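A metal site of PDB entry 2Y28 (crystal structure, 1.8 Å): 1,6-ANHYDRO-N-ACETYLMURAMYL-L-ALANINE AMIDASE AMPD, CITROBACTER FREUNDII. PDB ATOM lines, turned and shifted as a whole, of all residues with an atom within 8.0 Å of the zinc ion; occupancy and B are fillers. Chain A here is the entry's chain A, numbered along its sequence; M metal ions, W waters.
The side-chain carboxylate (OD2) of Asp 164 sits close to the backbone NH (N) of Asn 35, 3.1 Å away. A ring nitrogen (NE2) of His 154 lies within hydrogen-bond range of the backbone carbonyl oxygen of Ala 97 (2.8 Å). A ring nitrogen (NE2) of His 34 is in hydrogen-bond range of a ring nitrogen (ND1) of His 96 (2.8 Å). N of His 34 sits at hydrogen-bond distance from O of Ile 115, at 3.0 Å. O of Asp 164 lies within hydrogen-bond range of N of Cys 155 (2.8 Å). The backbone NH (N) of His 154 lies within hydrogen-bond range of the backbone carbonyl oxygen (O) of Val 33.
The side-chain carboxylate (OD2) of Asp 164 binds the zinc ion, at 2.0 Å. The zinc ion is bound by a ring nitrogen (ND1) of His 154 (2.0 Å). ND1 of His 34 is bound to the zinc ion, at 2.1 Å. Water W1 binds the zinc ion (2.1 Å). The zinc ion is bound by the side-chain carboxylate (OD1) of Asp 164, 2.5 Å away. The zinc ion has five donor atoms within binding distance.
Of the 20 residues printed, 3 come within 4 Å of the zinc ion.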
ATOM      1  N   VAL A  32      11.613   1.287   0.635  1.00  0.00           N
ATOM      2  CA  VAL A  32      10.304   1.643   1.155  1.00  0.00           C
ATOM      3  C   VAL A  32      10.465   2.526   2.375  1.00  0.00           C
ATOM      4  O   VAL A  32      11.093   2.114   3.363  1.00  0.00           O
ATOM      5  CB  VAL A  32       9.460   0.390   1.559  1.00  0.00           C
ATOM      6  CG1 VAL A  32       8.077   0.825   2.090  1.00  0.00           C
ATOM      7  CG2 VAL A  32       9.320  -0.582   0.394  1.00  0.00           C
ATOM      8  N   VAL A  33       9.911   3.742   2.328  1.00  0.00           N
ATOM      9  CA  VAL A  33       9.991   4.677   3.452  1.00  0.00           C
ATOM     10  C   VAL A  33       8.744   4.518   4.340  1.00  0.00           C
ATOM     11  O   VAL A  33       7.631   4.518   3.839  1.00  0.00           O
ATOM     12  CB  VAL A  33      10.126   6.131   2.953  1.00  0.00           C
ATOM     13  CG1 VAL A  33      10.238   7.092   4.126  1.00  0.00           C
ATOM     14  CG2 VAL A  33      11.334   6.258   2.030  1.00  0.00           C
ATOM     15  N   HIS A  34       8.959   4.362   5.648  1.00  0.00           N
ATOM     16  CA  HIS A  34       7.876   4.170   6.615  1.00  0.00           C
ATOM     17  C   HIS A  34       7.953   5.256   7.684  1.00  0.00           C
ATOM     18  O   HIS A  34       8.936   5.971   7.773  1.00  0.00           O
ATOM     19  CB  HIS A  34       8.050   2.837   7.360  1.00  0.00           C
ATOM     20  CG  HIS A  34       7.980   1.616   6.501  1.00  0.00           C
ATOM     21  ND1 HIS A  34       6.822   0.876   6.334  1.00  0.00           N
ATOM     22  CD2 HIS A  34       8.952   0.926   5.854  1.00  0.00           C
ATOM     23  CE1 HIS A  34       7.076  -0.161   5.565  1.00  0.00           C
ATOM     24  NE2 HIS A  34       8.358  -0.164   5.269  1.00  0.00           N
ATOM     25  N   ASN A  35       6.926   5.345   8.518  1.00  0.00           N
ATOM     26  CA  ASN A  35       7.113   6.059   9.779  1.00  0.00           C
ATOM     27  C   ASN A  35       6.605   5.245  10.955  1.00  0.00           C
ATOM     28  O   ASN A  35       5.888   4.273  10.777  1.00  0.00           O
ATOM     29  CB  ASN A  35       6.531   7.490   9.762  1.00  0.00           C
ATOM     30  CG  ASN A  35       5.006   7.527   9.720  1.00  0.00           C
ATOM     31  OD1 ASN A  35       4.325   6.578  10.108  1.00  0.00           O
ATOM     32  ND2 ASN A  35       4.472   8.636   9.204  1.00  0.00           N
ATOM     33  N   ILE A  36       6.988   5.625  12.156  1.00  0.00           N
ATOM     34  CA  ILE A  36       6.549   4.870  13.316  1.00  0.00           C
ATOM     35  C   ILE A  36       6.726   5.730  14.550  1.00  0.00           C
ATOM     36  O   ILE A  36       7.583   6.602  14.573  1.00  0.00           O
ATOM     37  CB  ILE A  36       7.323   3.532  13.447  1.00  0.00           C
ATOM     38  CG1 ILE A  36       6.721   2.677  14.569  1.00  0.00           C
ATOM     39  CG2 ILE A  36       8.796   3.792  13.649  1.00  0.00           C
ATOM     40  CD1 ILE A  36       7.210   1.245  14.596  1.00  0.00           C
ATOM     41  N   HIS A  96       8.599  -5.651   7.131  1.00  0.00           N
ATOM     42  CA  HIS A  96       8.175  -4.258   7.265  1.00  0.00           C
ATOM     43  C   HIS A  96       7.036  -3.802   6.337  1.00  0.00           C
ATOM     44  O   HIS A  96       6.396  -2.792   6.609  1.00  0.00           O
ATOM     45  CB  HIS A  96       9.379  -3.345   7.037  1.00  0.00           C
ATOM     46  CG  HIS A  96       9.937  -3.445   5.652  1.00  0.00           C
ATOM     47  ND1 HIS A  96       9.487  -2.660   4.613  1.00  0.00           N
ATOM     48  CD2 HIS A  96      10.873  -4.260   5.118  1.00  0.00           C
ATOM     49  CE1 HIS A  96      10.141  -2.976   3.506  1.00  0.00           C
ATOM     50  NE2 HIS A  96      10.985  -3.949   3.787  1.00  0.00           N
ATOM     51  N   ALA A  97       6.805  -4.532   5.248  1.00  0.00           N
ATOM     52  CA  ALA A  97       5.855  -4.079   4.222  1.00  0.00           C
ATOM     53  C   ALA A  97       4.512  -4.799   4.266  1.00  0.00           C
ATOM     54  O   ALA A  97       3.498  -4.278   3.802  1.00  0.00           O
ATOM     55  CB  ALA A  97       6.458  -4.251   2.835  1.00  0.00           C
ATOM     56  N   GLY A  98       4.510  -6.012   4.813  1.00  0.00           N
ATOM     57  CA  GLY A  98       3.310  -6.826   4.851  1.00  0.00           C
ATOM     58  C   GLY A  98       2.726  -7.084   3.453  1.00  0.00           C
ATOM     59  O   GLY A  98       3.455  -7.138   2.459  1.00  0.00           O
ATOM     60  N   ILE A 115      13.065   1.423   5.591  1.00  0.00           N
ATOM     61  CA  ILE A 115      13.674   2.371   6.507  1.00  0.00           C
ATOM     62  C   ILE A 115      12.576   3.130   7.201  1.00  0.00           C
ATOM     63  O   ILE A 115      11.716   3.737   6.535  1.00  0.00           O
ATOM     64  CB  ILE A 115      14.577   3.403   5.787  1.00  0.00           C
ATOM     65  CG1 ILE A 115      15.653   2.710   4.946  1.00  0.00           C
ATOM     66  CG2 ILE A 115      15.183   4.380   6.803  1.00  0.00           C
ATOM     67  CD1 ILE A 115      16.676   1.908   5.754  1.00  0.00           C
ATOM     68  N   GLU A 116      12.612   3.129   8.530  1.00  0.00           N
ATOM     69  CA  GLU A 116      11.603   3.790   9.348  1.00  0.00           C
ATOM     70  C   GLU A 116      12.028   5.180   9.801  1.00  0.00           C
ATOM     71  O   GLU A 116      13.095   5.331  10.390  1.00  0.00           O
ATOM     72  CB  GLU A 116      11.320   2.940  10.594  1.00  0.00           C
ATOM     73  CG  GLU A 116      10.606   1.639  10.300  1.00  0.00           C
ATOM     74  CD  GLU A 116       9.120   1.806  10.350  1.00  0.00           C
ATOM     75  OE1 GLU A 116       8.647   2.971  10.342  1.00  0.00           O
ATOM     76  OE2 GLU A 116       8.412   0.792  10.378  1.00  0.00           O
ATOM     77  N   GLY A 153       6.809   5.104  -0.820  1.00  0.00           N
ATOM     78  CA  GLY A 153       6.274   5.070   0.521  1.00  0.00           C
ATOM     79  C   GLY A 153       5.489   3.792   0.753  1.00  0.00           C
ATOM     80  O   GLY A 153       4.996   3.184  -0.178  1.00  0.00           O
ATOM     81  N   HIS A 154       5.410   3.370   2.011  1.00  0.00           N
ATOM     82  CA  HIS A 154       4.613   2.190   2.351  1.00  0.00           C
ATOM     83  C   HIS A 154       3.174   2.388   1.819  1.00  0.00           C
ATOM     84  O   HIS A 154       2.543   1.472   1.307  1.00  0.00           O
ATOM     85  CB  HIS A 154       4.654   1.944   3.854  1.00  0.00           C
ATOM     86  CG  HIS A 154       4.204   0.572   4.258  1.00  0.00           C
ATOM     87  ND1 HIS A 154       4.144   0.160   5.572  1.00  0.00           N
ATOM     88  CD2 HIS A 154       3.784  -0.480   3.519  1.00  0.00           C
ATOM     89  CE1 HIS A 154       3.718  -1.095   5.616  1.00  0.00           C
ATOM     90  NE2 HIS A 154       3.492  -1.501   4.388  1.00  0.00           N
ATOM     91  N   CYS A 155       2.692   3.628   1.897  1.00  0.00           N
ATOM     92  CA  CYS A 155       1.347   3.942   1.427  1.00  0.00           C
ATOM     93  C   CYS A 155       1.181   3.691  -0.077  1.00  0.00           C
ATOM     94  O   CYS A 155       0.073   3.460  -0.552  1.00  0.00           O
ATOM     95  CB  CYS A 155       1.003   5.403   1.750  1.00  0.00           C
ATOM     96  SG  CYS A 155       2.106   6.644   1.040  1.00  0.00           S
ATOM     97  N   ILE A 157       2.629   1.169  -1.797  1.00  0.00           N
ATOM     98  CA  ILE A 157       2.599  -0.261  -2.094  1.00  0.00           C
ATOM     99  C   ILE A 157       1.489  -0.982  -1.329  1.00  0.00           C
ATOM    100  O   ILE A 157       1.213  -2.150  -1.586  1.00  0.00           O
ATOM    101  CB  ILE A 157       3.969  -0.944  -1.862  1.00  0.00           C
ATOM    102  CG1 ILE A 157       4.403  -0.858  -0.397  1.00  0.00           C
ATOM    103  CG2 ILE A 157       5.029  -0.318  -2.754  1.00  0.00           C
ATOM    104  CD1 ILE A 157       5.736  -1.557  -0.114  1.00  0.00           C
ATOM    105  N   ALA A 158       0.846  -0.278  -0.395  1.00  0.00           N
ATOM    106  CA  ALA A 158      -0.250  -0.832   0.392  1.00  0.00           C
ATOM    107  C   ALA A 158      -1.340   0.214   0.594  1.00  0.00           C
ATOM    108  O   ALA A 158      -1.737   0.498   1.727  1.00  0.00           O
ATOM    109  CB  ALA A 158       0.255  -1.333   1.736  1.00  0.00           C
ATOM    110  N   ARG A 161      -4.451   0.490   3.047  1.00  0.00           N
ATOM    111  CA  ARG A 161      -4.077  -0.222   4.252  1.00  0.00           C
ATOM    112  C   ARG A 161      -3.120   0.639   5.064  1.00  0.00           C
ATOM    113  O   ARG A 161      -3.269   0.776   6.287  1.00  0.00           O
ATOM    114  CB  ARG A 161      -3.458  -1.577   3.921  1.00  0.00           C
ATOM    115  CG  ARG A 161      -3.467  -2.546   5.079  1.00  0.00           C
ATOM    116  CD  ARG A 161      -3.066  -3.952   4.656  1.00  0.00           C
ATOM    117  NE  ARG A 161      -1.677  -4.018   4.214  1.00  0.00           N
ATOM    118  CZ  ARG A 161      -0.641  -3.977   5.044  1.00  0.00           C
ATOM    119  NH1 ARG A 161      -0.841  -3.849   6.346  1.00  0.00           N
ATOM    120  NH2 ARG A 161       0.600  -4.034   4.564  1.00  0.00           N
ATOM    121  N   LYS A 162      -2.145   1.239   4.387  1.00  0.00           N
ATOM    122  CA  LYS A 162      -1.150   2.052   5.077  1.00  0.00           C
ATOM    123  C   LYS A 162      -1.146   3.490   4.582  1.00  0.00           C
ATOM    124  O   LYS A 162      -1.399   3.768   3.404  1.00  0.00           O
ATOM    125  CB  LYS A 162       0.244   1.429   4.926  1.00  0.00           C
ATOM    126  CG  LYS A 162       0.311  -0.052   5.299  1.00  0.00           C
ATOM    127  CD  LYS A 162      -0.072  -0.303   6.752  1.00  0.00           C
ATOM    128  CE  LYS A 162       0.985   0.198   7.699  1.00  0.00           C
ATOM    129  NZ  LYS A 162       0.691  -0.214   9.120  1.00  0.00           N
ATOM    130  N   THR A 163      -0.817   4.413   5.479  1.00  0.00           N
ATOM    131  CA  THR A 163      -0.752   5.818   5.137  1.00  0.00           C
ATOM    132  C   THR A 163       0.660   6.359   5.287  1.00  0.00           C
ATOM    133  O   THR A 163       0.963   7.433   4.778  1.00  0.00           O
ATOM    134  CB  THR A 163      -1.700   6.666   6.025  1.00  0.00           C
ATOM    135  OG1 THR A 163      -1.384   6.446   7.406  1.00  0.00           O
ATOM    136  CG2 THR A 163      -3.152   6.295   5.757  1.00  0.00           C
ATOM    137  N   ASP A 164       1.532   5.623   5.994  1.00  0.00           N
ATOM    138  CA  ASP A 164       2.902   6.085   6.230  1.00  0.00           C
ATOM    139  C   ASP A 164       3.700   6.116   4.938  1.00  0.00           C
ATOM    140  O   ASP A 164       3.470   5.280   4.074  1.00  0.00           O
ATOM    141  CB  ASP A 164       3.612   5.268   7.366  1.00  0.00           C
ATOM    142  CG  ASP A 164       3.896   3.787   7.003  1.00  0.00           C
ATOM    143  OD1 ASP A 164       3.011   3.000   6.649  1.00  0.00           O
ATOM    144  OD2 ASP A 164       5.042   3.342   7.138  1.00  0.00           O
ATOM    145  N   PRO A 165       4.634   7.084   4.782  1.00  0.00           N
ATOM    146  CA  PRO A 165       5.089   8.127   5.712  1.00  0.00           C
ATOM    147  C   PRO A 165       4.236   9.388   5.688  1.00  0.00           C
ATOM    148  O   PRO A 165       4.605  10.387   6.309  1.00  0.00           O
ATOM    149  CB  PRO A 165       6.489   8.455   5.202  1.00  0.00           C
ATOM    150  CG  PRO A 165       6.399   8.217   3.724  1.00  0.00           C
ATOM    151  CD  PRO A 165       5.455   7.044   3.560  1.00  0.00           C
HETATM  152 ZN    ZN M   1       4.871   1.375   7.018  1.00  0.00          ZN
HETATM  153  O   HOH W   1       4.425   0.396   8.869  1.00  0.00           O
